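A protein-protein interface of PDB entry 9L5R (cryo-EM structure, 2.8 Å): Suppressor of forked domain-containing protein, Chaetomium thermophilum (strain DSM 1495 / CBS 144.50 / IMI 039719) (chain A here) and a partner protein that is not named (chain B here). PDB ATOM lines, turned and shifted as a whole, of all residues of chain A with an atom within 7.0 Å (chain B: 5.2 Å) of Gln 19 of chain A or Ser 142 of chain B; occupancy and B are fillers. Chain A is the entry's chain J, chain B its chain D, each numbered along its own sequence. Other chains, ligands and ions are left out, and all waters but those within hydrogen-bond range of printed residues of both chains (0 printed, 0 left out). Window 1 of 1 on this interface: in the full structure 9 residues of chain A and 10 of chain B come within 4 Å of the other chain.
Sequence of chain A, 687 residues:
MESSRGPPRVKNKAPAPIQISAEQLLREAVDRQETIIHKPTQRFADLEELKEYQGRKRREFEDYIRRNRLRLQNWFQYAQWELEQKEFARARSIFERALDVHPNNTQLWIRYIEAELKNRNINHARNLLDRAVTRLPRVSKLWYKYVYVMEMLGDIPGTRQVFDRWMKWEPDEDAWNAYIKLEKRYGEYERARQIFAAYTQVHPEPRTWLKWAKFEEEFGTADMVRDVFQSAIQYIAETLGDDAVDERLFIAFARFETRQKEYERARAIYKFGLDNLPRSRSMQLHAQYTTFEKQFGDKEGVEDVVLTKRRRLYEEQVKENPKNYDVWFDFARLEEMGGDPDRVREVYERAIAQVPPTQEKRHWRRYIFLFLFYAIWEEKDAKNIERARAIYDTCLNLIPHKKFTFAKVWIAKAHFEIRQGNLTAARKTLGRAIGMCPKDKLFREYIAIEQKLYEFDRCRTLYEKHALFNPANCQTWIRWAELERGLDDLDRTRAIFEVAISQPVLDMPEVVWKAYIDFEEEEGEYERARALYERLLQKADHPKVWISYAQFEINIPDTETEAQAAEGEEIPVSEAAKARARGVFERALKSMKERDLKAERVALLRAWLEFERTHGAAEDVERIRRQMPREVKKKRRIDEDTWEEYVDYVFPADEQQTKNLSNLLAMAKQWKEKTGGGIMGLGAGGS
Hydrophobic or aromatic side chains of chain A within 4 Å of the printed part of chain B: Pro 15, Ile 18 and Ile 20.
Of the 10 printed residues of chain B, 9 touch a printed residue of chain A.
Hydrophobic or aromatic side chains of chain B that line the printed part of chain A: Leu 145 and Leu 150.
Among the printed residues, 23 pairs touch across the chains.
Among the printed residues, merely in contact across the chains: Gln 19 of chain A with Ser 142 of chain B, Ala 16 of chain A with Leu 145 of chain B, Gln 24 of chain A with Ser 142 of chain B, Ile 18 of chain A with Gln 139 of chain B, Gln 24 of chain A with Gln 139 of chain B, Ile 18 of chain A with Arg 143 of chain B, Pro 17 of chain A with Leu 145 of chain B, Ser 21 of chain A with Arg 143 of chain B, Ile 18 of chain A with Ser 142 of chain B, Ile 20 of chain A with Ser 142 of chain B, Pro 17 of chain A with Arg 143 of chain B, Gln 19 of chain A with Asn 144 of chain B, Ser 21 of chain A with Ser 142 of chain B, Ile 18 of chain A with Leu 150 of chain B, Pro 17 of chain A with Asn 144 of chain B, Gln 24 of chain A with Gly 140 of chain B, Ile 20 of chain A with Gln 139 of chain B and Pro 15 of chain A with Leu 145 of chain B.
OE1 of Gln 24 of chain A sits at hydrogen-bond distance from N of Ser 141 of chain B (3.4 Å).
O of Gln 19 of chain A is in hydrogen-bond range of N of Arg 143 of chain B (2.8 Å).
OE1 of Glu 23 of chain A lies within salt-bridge range of NH2 of Arg 149 of chain B (3.4 Å).
The side-chain hydroxyl of Ser 21 of chain A lies within hydrogen-bond range of the guanidinium group of Arg 149 of chain B (3.2 Å).
The side-chain hydroxyl (OG) of Ser 21 of chain A sits at hydrogen-bond distance from the backbone carbonyl oxygen (O) of Ser 141 of chain B (2.5 Å).
The side-chain amide nitrogen (NE2) of Gln 24 of chain A lies within hydrogen-bond range of the side-chain carboxylate (OE2) of Glu 28 of chain A (3.0 Å).
The backbone carbonyl oxygen (O) of Ala 16 of chain A lies within hydrogen-bond range of the side-chain amide nitrogen (NE2) of Gln 19 of chain A.
N of Gln 24 of chain A sits at hydrogen-bond distance from OG of Ser 21 of chain A (3.4 Å).
The backbone carbonyl oxygen (O) of Ser 142 of chain B lies within hydrogen-bond range of the backbone NH (N) of Leu 150 of chain B (3.2 Å).
The side-chain hydroxyl (OG) of Ser 142 of chain B sits at hydrogen-bond distance from the side-chain amide oxygen (OE1) of Gln 139 of chain B (3.1 Å).
The backbone carbonyl oxygen of Ser 141 of chain B sits at hydrogen-bond distance from the guanidinium group of Arg 149 of chain B (2.7 Å).
Ala 14 of chain A touches none of the printed residues of chain B.
Printed residues of chain B within 4 Å of Ala 16 of chain A: Leu 145 (3.3 Å).
Of the printed residues of chain B, Pro 17 of chain A touches Arg 143 (3.8 Å), Asn 144 (3.9 Å) and Leu 145 (3.6 Å).
Printed residues of chain B within 4 Å of Gln 19 of chain A: Ser 142 (3.2 Å), Arg 143 (2.8 Å) and Asn 144 (3.8 Å).
Of the printed residues of chain B, Ile 20 of chain A touches Gln 139 (3.9 Å) and Ser 142 (3.7 Å).
Leu 25 of chain A touches none of the printed residues of chain B.
Printed residues of chain A within 4 Å of Ser 141 of chain B: Ser 21 and Gln 24.
Ser 142 of chain B touches just these residues of chain A: Ile 18 (3.6 Å), Gln 19 (3.2 Å), Ile 20 (3.7 Å), Ser 21 (3.8 Å) and Gln 24 (3.4 Å).
Of the printed residues of chain A, Leu 150 of chain B touches Ile 18.
The nearest residue of chain B that does not touch Gln 19 of chain A is Leu 145 of chain B (4.8 Å).
The nearest residue of chain A that does not touch Ser 142 of chain B is Glu 28 of chain A (5.9 Å).
The nearest printed residue of chain B that does not touch Gln 24 of chain A is Arg 149 of chain B (5.3 Å).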
ATOM      1  N   ALA A  14     -33.709 -27.334  -4.043  1.00  0.00           N
ATOM      2  CA  ALA A  14     -33.100 -28.254  -3.098  1.00  0.00           C
ATOM      3  C   ALA A  14     -32.550 -27.469  -1.910  1.00  0.00           C
ATOM      4  O   ALA A  14     -32.088 -26.339  -2.084  1.00  0.00           O
ATOM      5  CB  ALA A  14     -31.984 -29.047  -3.772  1.00  0.00           C
ATOM      6  N   PRO A  15     -32.602 -28.027  -0.699  1.00  0.00           N
ATOM      7  CA  PRO A  15     -32.167 -27.271   0.485  1.00  0.00           C
ATOM      8  C   PRO A  15     -30.683 -26.936   0.439  1.00  0.00           C
ATOM      9  O   PRO A  15     -29.850 -27.770   0.084  1.00  0.00           O
ATOM     10  CB  PRO A  15     -32.497 -28.215   1.647  1.00  0.00           C
ATOM     11  CG  PRO A  15     -32.602 -29.555   1.041  1.00  0.00           C
ATOM     12  CD  PRO A  15     -33.146 -29.343  -0.333  1.00  0.00           C
ATOM     13  N   ALA A  16     -30.365 -25.695   0.796  1.00  0.00           N
ATOM     14  CA  ALA A  16     -29.001 -25.209   0.713  1.00  0.00           C
ATOM     15  C   ALA A  16     -28.117 -25.902   1.746  1.00  0.00           C
ATOM     16  O   ALA A  16     -28.579 -26.244   2.836  1.00  0.00           O
ATOM     17  CB  ALA A  16     -28.962 -23.700   0.920  1.00  0.00           C
ATOM     18  N   PRO A  17     -26.846 -26.151   1.414  1.00  0.00           N
ATOM     19  CA  PRO A  17     -25.937 -26.732   2.412  1.00  0.00           C
ATOM     20  C   PRO A  17     -25.688 -25.826   3.604  1.00  0.00           C
ATOM     21  O   PRO A  17     -25.481 -26.327   4.715  1.00  0.00           O
ATOM     22  CB  PRO A  17     -24.655 -26.984   1.609  1.00  0.00           C
ATOM     23  CG  PRO A  17     -24.715 -25.993   0.507  1.00  0.00           C
ATOM     24  CD  PRO A  17     -26.162 -25.918   0.132  1.00  0.00           C
ATOM     25  N   ILE A  18     -25.713 -24.514   3.408  1.00  0.00           N
ATOM     26  CA  ILE A  18     -25.462 -23.540   4.460  1.00  0.00           C
ATOM     27  C   ILE A  18     -26.760 -22.792   4.719  1.00  0.00           C
ATOM     28  O   ILE A  18     -27.338 -22.204   3.798  1.00  0.00           O
ATOM     29  CB  ILE A  18     -24.337 -22.570   4.068  1.00  0.00           C
ATOM     30  CG1 ILE A  18     -22.980 -23.262   4.149  1.00  0.00           C
ATOM     31  CG2 ILE A  18     -24.346 -21.353   4.953  1.00  0.00           C
ATOM     32  CD1 ILE A  18     -21.891 -22.503   3.447  1.00  0.00           C
ATOM     33  N   GLN A  19     -27.222 -22.820   5.963  1.00  0.00           N
ATOM     34  CA  GLN A  19     -28.424 -22.107   6.372  1.00  0.00           C
ATOM     35  C   GLN A  19     -28.028 -20.875   7.168  1.00  0.00           C
ATOM     36  O   GLN A  19     -27.274 -20.982   8.138  1.00  0.00           O
ATOM     37  CB  GLN A  19     -29.335 -23.007   7.205  1.00  0.00           C
ATOM     38  CG  GLN A  19     -29.769 -24.265   6.499  1.00  0.00           C
ATOM     39  CD  GLN A  19     -30.627 -23.979   5.293  1.00  0.00           C
ATOM     40  OE1 GLN A  19     -31.733 -23.470   5.413  1.00  0.00           O
ATOM     41  NE2 GLN A  19     -30.118 -24.305   4.120  1.00  0.00           N
ATOM     42  N   ILE A  20     -28.553 -19.711   6.762  1.00  0.00           N
ATOM     43  CA  ILE A  20     -28.251 -18.447   7.436  1.00  0.00           C
ATOM     44  C   ILE A  20     -28.718 -18.498   8.892  1.00  0.00           C
ATOM     45  O   ILE A  20     -29.580 -19.297   9.274  1.00  0.00           O
ATOM     46  CB  ILE A  20     -28.906 -17.279   6.678  1.00  0.00           C
ATOM     47  CG1 ILE A  20     -28.274 -15.929   7.023  1.00  0.00           C
ATOM     48  CG2 ILE A  20     -30.389 -17.217   6.961  1.00  0.00           C
ATOM     49  CD1 ILE A  20     -26.926 -15.720   6.451  1.00  0.00           C
ATOM     50  N   SER A  21     -28.096 -17.668   9.724  1.00  0.00           N
ATOM     51  CA  SER A  21     -28.500 -17.524  11.109  1.00  0.00           C
ATOM     52  C   SER A  21     -28.455 -16.054  11.495  1.00  0.00           C
ATOM     53  O   SER A  21     -27.859 -15.219  10.806  1.00  0.00           O
ATOM     54  CB  SER A  21     -27.623 -18.354  12.047  1.00  0.00           C
ATOM     55  OG  SER A  21     -26.306 -17.853  12.084  1.00  0.00           O
ATOM     56  N   GLU A  23     -26.972 -14.669  14.033  1.00  0.00           N
ATOM     57  CA  GLU A  23     -25.622 -14.236  14.372  1.00  0.00           C
ATOM     58  C   GLU A  23     -24.786 -13.973  13.130  1.00  0.00           C
ATOM     59  O   GLU A  23     -23.955 -13.060  13.131  1.00  0.00           O
ATOM     60  CB  GLU A  23     -24.966 -15.282  15.260  1.00  0.00           C
ATOM     61  CG  GLU A  23     -25.466 -15.257  16.688  1.00  0.00           C
ATOM     62  CD  GLU A  23     -26.770 -16.011  16.883  1.00  0.00           C
ATOM     63  OE1 GLU A  23     -27.380 -16.451  15.887  1.00  0.00           O
ATOM     64  OE2 GLU A  23     -27.190 -16.170  18.049  1.00  0.00           O
ATOM     65  N   GLN A  24     -24.998 -14.747  12.063  1.00  0.00           N
ATOM     66  CA  GLN A  24     -24.342 -14.463  10.793  1.00  0.00           C
ATOM     67  C   GLN A  24     -24.803 -13.132  10.227  1.00  0.00           C
ATOM     68  O   GLN A  24     -23.994 -12.362   9.691  1.00  0.00           O
ATOM     69  CB  GLN A  24     -24.616 -15.591   9.800  1.00  0.00           C
ATOM     70  CG  GLN A  24     -23.868 -15.469   8.479  1.00  0.00           C
ATOM     71  CD  GLN A  24     -22.367 -15.441   8.655  1.00  0.00           C
ATOM     72  OE1 GLN A  24     -21.818 -16.138   9.498  1.00  0.00           O
ATOM     73  NE2 GLN A  24     -21.696 -14.628   7.858  1.00  0.00           N
ATOM     74  N   LEU A  25     -26.103 -12.841  10.344  1.00  0.00           N
ATOM     75  CA  LEU A  25     -26.625 -11.539   9.932  1.00  0.00           C
ATOM     76  C   LEU A  25     -25.991 -10.402  10.722  1.00  0.00           C
ATOM     77  O   LEU A  25     -25.630  -9.368  10.152  1.00  0.00           O
ATOM     78  CB  LEU A  25     -28.134 -11.506  10.113  1.00  0.00           C
ATOM     79  CG  LEU A  25     -28.977 -12.254   9.099  1.00  0.00           C
ATOM     80  CD1 LEU A  25     -30.384 -12.356   9.618  1.00  0.00           C
ATOM     81  CD2 LEU A  25     -28.936 -11.524   7.783  1.00  0.00           C
ATOM     82  N   GLU A  28     -22.414  -9.867   9.569  1.00  0.00           N
ATOM     83  CA  GLU A  28     -22.376  -9.162   8.295  1.00  0.00           C
ATOM     84  C   GLU A  28     -22.734  -7.687   8.452  1.00  0.00           C
ATOM     85  O   GLU A  28     -22.165  -6.836   7.763  1.00  0.00           O
ATOM     86  CB  GLU A  28     -23.298  -9.851   7.301  1.00  0.00           C
ATOM     87  CG  GLU A  28     -22.740 -11.156   6.787  1.00  0.00           C
ATOM     88  CD  GLU A  28     -23.814 -12.103   6.313  1.00  0.00           C
ATOM     89  OE1 GLU A  28     -24.994 -11.705   6.300  1.00  0.00           O
ATOM     90  OE2 GLU A  28     -23.483 -13.249   5.949  1.00  0.00           O
ATOM     91  N   GLN B 139     -18.698 -17.774   6.803  1.00  0.00           N
ATOM     92  CA  GLN B 139     -20.041 -18.104   7.265  1.00  0.00           C
ATOM     93  C   GLN B 139     -20.013 -19.053   8.457  1.00  0.00           C
ATOM     94  O   GLN B 139     -20.858 -19.937   8.583  1.00  0.00           O
ATOM     95  CB  GLN B 139     -20.867 -18.691   6.128  1.00  0.00           C
ATOM     96  CG  GLN B 139     -21.444 -17.635   5.208  1.00  0.00           C
ATOM     97  CD  GLN B 139     -22.753 -18.054   4.573  1.00  0.00           C
ATOM     98  OE1 GLN B 139     -23.832 -17.753   5.085  1.00  0.00           O
ATOM     99  NE2 GLN B 139     -22.666 -18.743   3.441  1.00  0.00           N
ATOM    100  N   GLY B 140     -19.034 -18.861   9.347  1.00  0.00           N
ATOM    101  CA  GLY B 140     -18.858 -19.752  10.482  1.00  0.00           C
ATOM    102  C   GLY B 140     -20.016 -19.784  11.461  1.00  0.00           C
ATOM    103  O   GLY B 140     -20.204 -20.775  12.167  1.00  0.00           O
ATOM    104  N   SER B 141     -20.803 -18.720  11.527  1.00  0.00           N
ATOM    105  CA  SER B 141     -21.946 -18.700  12.427  1.00  0.00           C
ATOM    106  C   SER B 141     -23.220 -19.221  11.786  1.00  0.00           C
ATOM    107  O   SER B 141     -24.248 -19.294  12.462  1.00  0.00           O
ATOM    108  CB  SER B 141     -22.176 -17.292  12.962  1.00  0.00           C
ATOM    109  OG  SER B 141     -21.101 -16.893  13.790  1.00  0.00           O
ATOM    110  N   SER B 142     -23.180 -19.592  10.511  1.00  0.00           N
ATOM    111  CA  SER B 142     -24.326 -20.187   9.849  1.00  0.00           C
ATOM    112  C   SER B 142     -24.453 -21.653  10.250  1.00  0.00           C
ATOM    113  O   SER B 142     -23.637 -22.187  10.998  1.00  0.00           O
ATOM    114  CB  SER B 142     -24.197 -20.027   8.343  1.00  0.00           C
ATOM    115  OG  SER B 142     -24.581 -18.730   7.944  1.00  0.00           O
ATOM    116  N   ARG B 143     -25.472 -22.328   9.739  1.00  0.00           N
ATOM    117  CA  ARG B 143     -25.780 -23.674  10.193  1.00  0.00           C
ATOM    118  C   ARG B 143     -25.743 -24.679   9.047  1.00  0.00           C
ATOM    119  O   ARG B 143     -25.905 -24.331   7.875  1.00  0.00           O
ATOM    120  CB  ARG B 143     -27.148 -23.718  10.872  1.00  0.00           C
ATOM    121  CG  ARG B 143     -27.122 -23.252  12.298  1.00  0.00           C
ATOM    122  CD  ARG B 143     -28.434 -23.535  12.973  1.00  0.00           C
ATOM    123  NE  ARG B 143     -28.431 -23.071  14.352  1.00  0.00           N
ATOM    124  CZ  ARG B 143     -28.832 -21.870  14.740  1.00  0.00           C
ATOM    125  NH1 ARG B 143     -29.281 -20.979  13.875  1.00  0.00           N
ATOM    126  NH2 ARG B 143     -28.783 -21.556  16.028  1.00  0.00           N
ATOM    127  N   ASN B 144     -25.527 -25.941   9.415  1.00  0.00           N
ATOM    128  CA  ASN B 144     -25.611 -27.075   8.504  1.00  0.00           C
ATOM    129  C   ASN B 144     -27.072 -27.464   8.306  1.00  0.00           C
ATOM    130  O   ASN B 144     -27.993 -26.754   8.713  1.00  0.00           O
ATOM    131  CB  ASN B 144     -24.819 -28.261   9.045  1.00  0.00           C
ATOM    132  CG  ASN B 144     -23.369 -28.229   8.652  1.00  0.00           C
ATOM    133  OD1 ASN B 144     -22.488 -28.218   9.505  1.00  0.00           O
ATOM    134  ND2 ASN B 144     -23.108 -28.227   7.352  1.00  0.00           N
ATOM    135  N   LEU B 145     -27.307 -28.617   7.679  1.00  0.00           N
ATOM    136  CA  LEU B 145     -28.663 -29.144   7.606  1.00  0.00           C
ATOM    137  C   LEU B 145     -29.095 -29.772   8.919  1.00  0.00           C
ATOM    138  O   LEU B 145     -30.291 -29.808   9.220  1.00  0.00           O
ATOM    139  CB  LEU B 145     -28.801 -30.187   6.500  1.00  0.00           C
ATOM    140  CG  LEU B 145     -29.033 -29.766   5.051  1.00  0.00           C
ATOM    141  CD1 LEU B 145     -30.365 -29.042   4.909  1.00  0.00           C
ATOM    142  CD2 LEU B 145     -27.892 -28.966   4.492  1.00  0.00           C
ATOM    143  N   ARG B 148     -26.179 -27.474  13.018  1.00  0.00           N
ATOM    144  CA  ARG B 148     -24.917 -27.301  13.717  1.00  0.00           C
ATOM    145  C   ARG B 148     -24.113 -26.201  13.050  1.00  0.00           C
ATOM    146  O   ARG B 148     -24.084 -26.100  11.822  1.00  0.00           O
ATOM    147  CB  ARG B 148     -24.140 -28.613  13.733  1.00  0.00           C
ATOM    148  CG  ARG B 148     -24.932 -29.679  14.441  1.00  0.00           C
ATOM    149  CD  ARG B 148     -25.028 -29.355  15.911  1.00  0.00           C
ATOM    150  NE  ARG B 148     -25.809 -30.340  16.643  1.00  0.00           N
ATOM    151  CZ  ARG B 148     -25.298 -31.427  17.195  1.00  0.00           C
ATOM    152  NH1 ARG B 148     -24.050 -31.782  16.980  1.00  0.00           N
ATOM    153  NH2 ARG B 148     -26.066 -32.188  17.965  1.00  0.00           N
ATOM    154  N   ARG B 149     -23.474 -25.369  13.865  1.00  0.00           N
ATOM    155  CA  ARG B 149     -22.723 -24.251  13.323  1.00  0.00           C
ATOM    156  C   ARG B 149     -21.430 -24.725  12.678  1.00  0.00           C
ATOM    157  O   ARG B 149     -20.748 -25.632  13.174  1.00  0.00           O
ATOM    158  CB  ARG B 149     -22.433 -23.221  14.409  1.00  0.00           C
ATOM    159  CG  ARG B 149     -23.673 -22.524  14.937  1.00  0.00           C
ATOM    160  CD  ARG B 149     -23.364 -21.138  15.446  1.00  0.00           C
ATOM    161  NE  ARG B 149     -24.391 -20.667  16.366  1.00  0.00           N
ATOM    162  CZ  ARG B 149     -25.309 -19.758  16.070  1.00  0.00           C
ATOM    163  NH1 ARG B 149     -25.357 -19.185  14.882  1.00  0.00           N
ATOM    164  NH2 ARG B 149     -26.197 -19.411  16.993  1.00  0.00           N
ATOM    165  N   LEU B 150     -21.107 -24.101  11.543  1.00  0.00           N
ATOM    166  CA  LEU B 150     -19.916 -24.473  10.789  1.00  0.00           C
ATOM    167  C   LEU B 150     -18.652 -24.216  11.590  1.00  0.00           C
ATOM    168  O   LEU B 150     -17.673 -24.966  11.472  1.00  0.00           O
ATOM    169  CB  LEU B 150     -19.872 -23.707   9.468  1.00  0.00           C
ATOM    170  CG  LEU B 150     -21.142 -23.678   8.618  1.00  0.00           C
ATOM    171  CD1 LEU B 150     -20.856 -23.030   7.287  1.00  0.00           C
ATOM    172  CD2 LEU B 150     -21.697 -25.064   8.408  1.00  0.00           C
